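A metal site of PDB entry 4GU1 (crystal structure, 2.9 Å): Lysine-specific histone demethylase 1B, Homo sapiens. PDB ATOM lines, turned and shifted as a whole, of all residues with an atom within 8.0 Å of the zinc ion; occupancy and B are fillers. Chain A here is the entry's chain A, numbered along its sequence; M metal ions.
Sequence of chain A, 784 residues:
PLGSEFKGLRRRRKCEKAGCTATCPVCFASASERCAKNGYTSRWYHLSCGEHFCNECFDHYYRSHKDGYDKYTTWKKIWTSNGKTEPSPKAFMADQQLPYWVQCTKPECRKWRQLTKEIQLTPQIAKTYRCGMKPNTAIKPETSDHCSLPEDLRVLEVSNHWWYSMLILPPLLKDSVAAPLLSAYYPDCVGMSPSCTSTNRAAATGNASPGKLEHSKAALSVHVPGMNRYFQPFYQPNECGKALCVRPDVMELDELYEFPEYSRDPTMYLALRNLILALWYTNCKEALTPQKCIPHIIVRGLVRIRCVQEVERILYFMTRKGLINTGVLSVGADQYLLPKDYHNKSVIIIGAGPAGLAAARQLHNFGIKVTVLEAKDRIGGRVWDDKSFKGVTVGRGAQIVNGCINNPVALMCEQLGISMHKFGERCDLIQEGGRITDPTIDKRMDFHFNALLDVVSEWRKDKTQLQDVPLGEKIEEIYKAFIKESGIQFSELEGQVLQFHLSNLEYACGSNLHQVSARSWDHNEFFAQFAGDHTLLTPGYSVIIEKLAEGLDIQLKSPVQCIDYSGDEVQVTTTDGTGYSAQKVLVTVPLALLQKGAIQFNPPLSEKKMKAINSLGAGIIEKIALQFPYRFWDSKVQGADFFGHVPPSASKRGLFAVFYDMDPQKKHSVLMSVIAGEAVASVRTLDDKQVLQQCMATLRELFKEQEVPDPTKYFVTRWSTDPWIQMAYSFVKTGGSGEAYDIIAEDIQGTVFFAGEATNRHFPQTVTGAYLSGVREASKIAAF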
ATOM      1  N   LYS A  14      -2.941  16.990   4.259  1.00  0.00           N
ATOM      2  CA  LYS A  14      -2.581  17.820   3.091  1.00  0.00           C
ATOM      3  C   LYS A  14      -2.163  17.037   1.822  1.00  0.00           C
ATOM      4  O   LYS A  14      -2.560  17.423   0.718  1.00  0.00           O
ATOM      5  CB  LYS A  14      -1.507  18.826   3.497  1.00  0.00           C
ATOM      6  CG  LYS A  14      -1.557  20.126   2.708  1.00  0.00           C
ATOM      7  CD  LYS A  14      -1.106  21.320   3.582  1.00  0.00           C
ATOM      8  CE  LYS A  14      -2.168  21.750   4.617  1.00  0.00           C
ATOM      9  NZ  LYS A  14      -1.555  22.246   5.891  1.00  0.00           N
ATOM     10  N   CYS A  15      -1.371  15.971   1.966  1.00  0.00           N
ATOM     11  CA  CYS A  15      -1.054  15.099   0.832  1.00  0.00           C
ATOM     12  C   CYS A  15      -2.115  14.025   0.696  1.00  0.00           C
ATOM     13  O   CYS A  15      -2.534  13.441   1.696  1.00  0.00           O
ATOM     14  CB  CYS A  15       0.320  14.425   1.001  1.00  0.00           C
ATOM     15  SG  CYS A  15       0.783  13.178  -0.274  1.00  0.00           S
ATOM     16  N   GLU A  16      -2.534  13.744  -0.522  1.00  0.00           N
ATOM     17  CA  GLU A  16      -3.595  12.771  -0.728  1.00  0.00           C
ATOM     18  C   GLU A  16      -3.175  11.322  -0.419  1.00  0.00           C
ATOM     19  O   GLU A  16      -3.951  10.569   0.184  1.00  0.00           O
ATOM     20  CB  GLU A  16      -4.180  12.871  -2.137  1.00  0.00           C
ATOM     21  CG  GLU A  16      -3.189  12.555  -3.244  1.00  0.00           C
ATOM     22  CD  GLU A  16      -3.885  12.083  -4.507  1.00  0.00           C
ATOM     23  OE1 GLU A  16      -3.342  11.179  -5.183  1.00  0.00           O
ATOM     24  OE2 GLU A  16      -4.976  12.629  -4.828  1.00  0.00           O
ATOM     25  N   LYS A  17      -1.956  10.937  -0.815  1.00  0.00           N
ATOM     26  CA  LYS A  17      -1.440   9.591  -0.584  1.00  0.00           C
ATOM     27  C   LYS A  17      -1.556   9.189   0.887  1.00  0.00           C
ATOM     28  O   LYS A  17      -1.182   9.943   1.784  1.00  0.00           O
ATOM     29  CB  LYS A  17       0.014   9.473  -1.049  1.00  0.00           C
ATOM     30  CG  LYS A  17       0.836   8.406  -0.306  1.00  0.00           C
ATOM     31  CD  LYS A  17       0.828   7.029  -0.975  1.00  0.00           C
ATOM     32  CE  LYS A  17       1.391   5.959  -0.029  1.00  0.00           C
ATOM     33  NZ  LYS A  17       2.039   4.805  -0.710  1.00  0.00           N
ATOM     34  N   ALA A  18      -2.081   7.986   1.104  1.00  0.00           N
ATOM     35  CA  ALA A  18      -2.343   7.483   2.453  1.00  0.00           C
ATOM     36  C   ALA A  18      -1.059   7.124   3.189  1.00  0.00           C
ATOM     37  O   ALA A  18      -0.321   6.232   2.754  1.00  0.00           O
ATOM     38  CB  ALA A  18      -3.261   6.281   2.392  1.00  0.00           C
ATOM     39  N   GLY A  19      -0.802   7.814   4.294  1.00  0.00           N
ATOM     40  CA  GLY A  19       0.307   7.465   5.157  1.00  0.00           C
ATOM     41  C   GLY A  19       1.555   8.322   5.009  1.00  0.00           C
ATOM     42  O   GLY A  19       2.589   8.028   5.632  1.00  0.00           O
ATOM     43  N   CYS A  20       1.460   9.367   4.177  1.00  0.00           N
ATOM     44  CA  CYS A  20       2.539  10.363   4.085  1.00  0.00           C
ATOM     45  C   CYS A  20       2.685  10.972   5.469  1.00  0.00           C
ATOM     46  O   CYS A  20       1.709  11.045   6.213  1.00  0.00           O
ATOM     47  CB  CYS A  20       2.224  11.449   3.051  1.00  0.00           C
ATOM     48  SG  CYS A  20       3.654  12.500   2.596  1.00  0.00           S
ATOM     49  N   THR A  21       3.900  11.366   5.806  1.00  0.00           N
ATOM     50  CA  THR A  21       4.188  11.851   7.155  1.00  0.00           C
ATOM     51  C   THR A  21       4.596  13.304   7.122  1.00  0.00           C
ATOM     52  O   THR A  21       4.990  13.879   8.133  1.00  0.00           O
ATOM     53  CB  THR A  21       5.288  11.015   7.833  1.00  0.00           C
ATOM     54  OG1 THR A  21       6.476  11.042   7.043  1.00  0.00           O
ATOM     55  CG2 THR A  21       4.841   9.592   8.018  1.00  0.00           C
ATOM     56  N   ALA A  22       4.530  13.893   5.929  1.00  0.00           N
ATOM     57  CA  ALA A  22       4.780  15.323   5.802  1.00  0.00           C
ATOM     58  C   ALA A  22       3.457  16.058   5.971  1.00  0.00           C
ATOM     59  O   ALA A  22       2.494  15.849   5.219  1.00  0.00           O
ATOM     60  CB  ALA A  22       5.429  15.648   4.470  1.00  0.00           C
ATOM     61  N   THR A  23       3.381  16.902   6.986  1.00  0.00           N
ATOM     62  CA  THR A  23       2.170  17.660   7.225  1.00  0.00           C
ATOM     63  C   THR A  23       2.239  18.985   6.466  1.00  0.00           C
ATOM     64  O   THR A  23       1.222  19.624   6.194  1.00  0.00           O
ATOM     65  CB  THR A  23       1.959  17.906   8.709  1.00  0.00           C
ATOM     66  OG1 THR A  23       2.992  18.776   9.199  1.00  0.00           O
ATOM     67  CG2 THR A  23       1.990  16.573   9.437  1.00  0.00           C
ATOM     68  N   PRO A  25       3.765  19.618   3.014  1.00  0.00           N
ATOM     69  CA  PRO A  25       4.333  19.368   1.709  1.00  0.00           C
ATOM     70  C   PRO A  25       4.740  20.696   1.103  1.00  0.00           C
ATOM     71  O   PRO A  25       3.868  21.472   0.745  1.00  0.00           O
ATOM     72  CB  PRO A  25       3.155  18.810   0.908  1.00  0.00           C
ATOM     73  CG  PRO A  25       2.166  18.375   1.894  1.00  0.00           C
ATOM     74  CD  PRO A  25       2.326  19.277   3.054  1.00  0.00           C
ATOM     75  N   TRP A  44      -1.659  17.863  -4.164  1.00  0.00           N
ATOM     76  CA  TRP A  44      -0.249  17.550  -4.011  1.00  0.00           C
ATOM     77  C   TRP A  44       0.085  16.225  -4.670  1.00  0.00           C
ATOM     78  O   TRP A  44      -0.761  15.327  -4.751  1.00  0.00           O
ATOM     79  CB  TRP A  44       0.147  17.523  -2.528  1.00  0.00           C
ATOM     80  CG  TRP A  44       0.372  18.878  -1.962  1.00  0.00           C
ATOM     81  CD1 TRP A  44      -0.385  19.502  -1.016  1.00  0.00           C
ATOM     82  CD2 TRP A  44       1.426  19.789  -2.295  1.00  0.00           C
ATOM     83  NE1 TRP A  44       0.140  20.742  -0.737  1.00  0.00           N
ATOM     84  CE2 TRP A  44       1.246  20.938  -1.514  1.00  0.00           C
ATOM     85  CE3 TRP A  44       2.505  19.739  -3.185  1.00  0.00           C
ATOM     86  CZ2 TRP A  44       2.102  22.035  -1.600  1.00  0.00           C
ATOM     87  CZ3 TRP A  44       3.358  20.824  -3.253  1.00  0.00           C
ATOM     88  CH2 TRP A  44       3.146  21.958  -2.465  1.00  0.00           C
ATOM     89  N   TYR A  45       1.310  16.096  -5.170  1.00  0.00           N
ATOM     90  CA  TYR A  45       1.739  14.839  -5.764  1.00  0.00           C
ATOM     91  C   TYR A  45       2.874  14.225  -4.970  1.00  0.00           C
ATOM     92  O   TYR A  45       3.896  14.866  -4.694  1.00  0.00           O
ATOM     93  CB  TYR A  45       2.109  15.014  -7.232  1.00  0.00           C
ATOM     94  CG  TYR A  45       0.893  15.262  -8.070  1.00  0.00           C
ATOM     95  CD1 TYR A  45       0.050  14.221  -8.402  1.00  0.00           C
ATOM     96  CD2 TYR A  45       0.551  16.534  -8.486  1.00  0.00           C
ATOM     97  CE1 TYR A  45      -1.082  14.426  -9.158  1.00  0.00           C
ATOM     98  CE2 TYR A  45      -0.579  16.753  -9.243  1.00  0.00           C
ATOM     99  CZ  TYR A  45      -1.395  15.699  -9.579  1.00  0.00           C
ATOM    100  OH  TYR A  45      -2.528  15.906 -10.317  1.00  0.00           O
ATOM    101  N   HIS A  46       2.665  12.966  -4.593  1.00  0.00           N
ATOM    102  CA  HIS A  46       3.581  12.275  -3.691  1.00  0.00           C
ATOM    103  C   HIS A  46       4.671  11.519  -4.463  1.00  0.00           C
ATOM    104  O   HIS A  46       4.383  10.672  -5.336  1.00  0.00           O
ATOM    105  CB  HIS A  46       2.799  11.316  -2.782  1.00  0.00           C
ATOM    106  CG  HIS A  46       3.637  10.638  -1.744  1.00  0.00           C
ATOM    107  ND1 HIS A  46       4.010  11.256  -0.570  1.00  0.00           N
ATOM    108  CD2 HIS A  46       4.187   9.402  -1.722  1.00  0.00           C
ATOM    109  CE1 HIS A  46       4.756  10.424   0.139  1.00  0.00           C
ATOM    110  NE2 HIS A  46       4.872   9.289  -0.541  1.00  0.00           N
ATOM    111  N   LEU A  47       5.934  11.841  -4.180  1.00  0.00           N
ATOM    112  CA  LEU A  47       7.030  11.077  -4.747  1.00  0.00           C
ATOM    113  C   LEU A  47       7.614  10.207  -3.654  1.00  0.00           C
ATOM    114  O   LEU A  47       7.617   8.986  -3.776  1.00  0.00           O
ATOM    115  CB  LEU A  47       8.093  11.993  -5.354  1.00  0.00           C
ATOM    116  CG  LEU A  47       8.152  11.902  -6.882  1.00  0.00           C
ATOM    117  CD1 LEU A  47       6.760  11.932  -7.492  1.00  0.00           C
ATOM    118  CD2 LEU A  47       9.003  13.015  -7.435  1.00  0.00           C
ATOM    119  N   SER A  48       8.081  10.852  -2.597  1.00  0.00           N
ATOM    120  CA  SER A  48       8.503  10.170  -1.384  1.00  0.00           C
ATOM    121  C   SER A  48       7.915  10.918  -0.198  1.00  0.00           C
ATOM    122  O   SER A  48       7.166  11.864  -0.379  1.00  0.00           O
ATOM    123  CB  SER A  48      10.024  10.136  -1.270  1.00  0.00           C
ATOM    124  OG  SER A  48      10.516  11.289  -0.634  1.00  0.00           O
ATOM    125  N   CYS A  49       8.254  10.511   1.012  1.00  0.00           N
ATOM    126  CA  CYS A  49       7.703  11.157   2.188  1.00  0.00           C
ATOM    127  C   CYS A  49       8.236  12.582   2.382  1.00  0.00           C
ATOM    128  O   CYS A  49       7.657  13.375   3.122  1.00  0.00           O
ATOM    129  CB  CYS A  49       7.980  10.332   3.436  1.00  0.00           C
ATOM    130  SG  CYS A  49       6.576   9.317   4.010  1.00  0.00           S
ATOM    131  N   GLY A  50       9.341  12.892   1.721  1.00  0.00           N
ATOM    132  CA  GLY A  50       9.934  14.209   1.825  1.00  0.00           C
ATOM    133  C   GLY A  50      10.128  14.840   0.465  1.00  0.00           C
ATOM    134  O   GLY A  50      11.016  15.697   0.290  1.00  0.00           O
ATOM    135  N   GLU A  51       9.304  14.444  -0.507  1.00  0.00           N
ATOM    136  CA  GLU A  51       9.411  14.985  -1.848  1.00  0.00           C
ATOM    137  C   GLU A  51       8.042  15.056  -2.513  1.00  0.00           C
ATOM    138  O   GLU A  51       7.458  14.025  -2.834  1.00  0.00           O
ATOM    139  CB  GLU A  51      10.381  14.164  -2.702  1.00  0.00           C
ATOM    140  CG  GLU A  51      11.844  14.612  -2.579  1.00  0.00           C
ATOM    141  CD  GLU A  51      12.878  13.451  -2.564  1.00  0.00           C
ATOM    142  OE1 GLU A  51      14.064  13.712  -2.927  1.00  0.00           O
ATOM    143  OE2 GLU A  51      12.525  12.320  -2.182  1.00  0.00           O
ATOM    144  N   HIS A  52       7.530  16.284  -2.685  1.00  0.00           N
ATOM    145  CA  HIS A  52       6.237  16.501  -3.330  1.00  0.00           C
ATOM    146  C   HIS A  52       6.333  17.570  -4.420  1.00  0.00           C
ATOM    147  O   HIS A  52       7.289  18.364  -4.448  1.00  0.00           O
ATOM    148  CB  HIS A  52       5.181  16.935  -2.319  1.00  0.00           C
ATOM    149  CG  HIS A  52       5.005  15.989  -1.174  1.00  0.00           C
ATOM    150  ND1 HIS A  52       5.891  15.920  -0.114  1.00  0.00           N
ATOM    151  CD2 HIS A  52       4.022  15.088  -0.897  1.00  0.00           C
ATOM    152  CE1 HIS A  52       5.471  14.996   0.743  1.00  0.00           C
ATOM    153  NE2 HIS A  52       4.342  14.480   0.293  1.00  0.00           N
ATOM    154  N   PHE A  53       5.353  17.594  -5.315  1.00  0.00           N
ATOM    155  CA  PHE A  53       5.245  18.693  -6.269  1.00  0.00           C
ATOM    156  C   PHE A  53       3.788  19.092  -6.514  1.00  0.00           C
ATOM    157  O   PHE A  53       2.896  18.243  -6.479  1.00  0.00           O
ATOM    158  CB  PHE A  53       6.013  18.407  -7.560  1.00  0.00           C
ATOM    159  CG  PHE A  53       5.424  17.328  -8.421  1.00  0.00           C
ATOM    160  CD1 PHE A  53       4.502  17.629  -9.402  1.00  0.00           C
ATOM    161  CD2 PHE A  53       5.822  16.019  -8.261  1.00  0.00           C
ATOM    162  CE1 PHE A  53       3.965  16.641 -10.203  1.00  0.00           C
ATOM    163  CE2 PHE A  53       5.287  15.022  -9.067  1.00  0.00           C
ATOM    164  CZ  PHE A  53       4.363  15.332 -10.043  1.00  0.00           C
ATOM    165  N   MET A 166       6.895   4.111   1.481  1.00  0.00           N
ATOM    166  CA  MET A 166       6.231   5.360   1.100  1.00  0.00           C
ATOM    167  C   MET A 166       6.803   5.966  -0.160  1.00  0.00           C
ATOM    168  O   MET A 166       6.299   6.970  -0.667  1.00  0.00           O
ATOM    169  CB  MET A 166       6.297   6.377   2.234  1.00  0.00           C
ATOM    170  CG  MET A 166       5.306   6.100   3.342  1.00  0.00           C
ATOM    171  SD  MET A 166       3.586   6.066   2.771  1.00  0.00           S
ATOM    172  CE  MET A 166       3.212   4.307   2.850  1.00  0.00           C
HETATM  173 ZN    ZN M   1       2.984  12.795   0.553  1.00  0.00          ZN
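The zinc ion is bound by ND1 of His 46, at 2.2 Å.
The zinc ion is bound by the side-chain sulfur (SG) of Cys 20 (2.2 Å).
NE2 of His 52 is bound to the zinc ion (2.2 Å).
The side-chain sulfur (SG) of Cys 15 is bound to the zinc ion, 2.4 Å away.
Four residues have an atom within 4 Å of the zinc ion: Cys 15, Cys 20, His 46 and His 52.
The nearest printed residue that does not touch the zinc ion is Ser 48 (4.4 Å).
The backbone carbonyl oxygen (O) of Ser 48 lies close to a ring nitrogen (NE2) of His 46, at 3.5 Å.
NE2 of His 46 lies within hydrogen-bond range of O of Met 166 (2.7 Å).
The side-chain sulfur of Cys 15 lies close to the backbone NH of Lys 17 (3.6 Å).
The backbone NH of Ala 22 sits close to the side-chain sulfur of Cys 20, 3.7 Å away.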
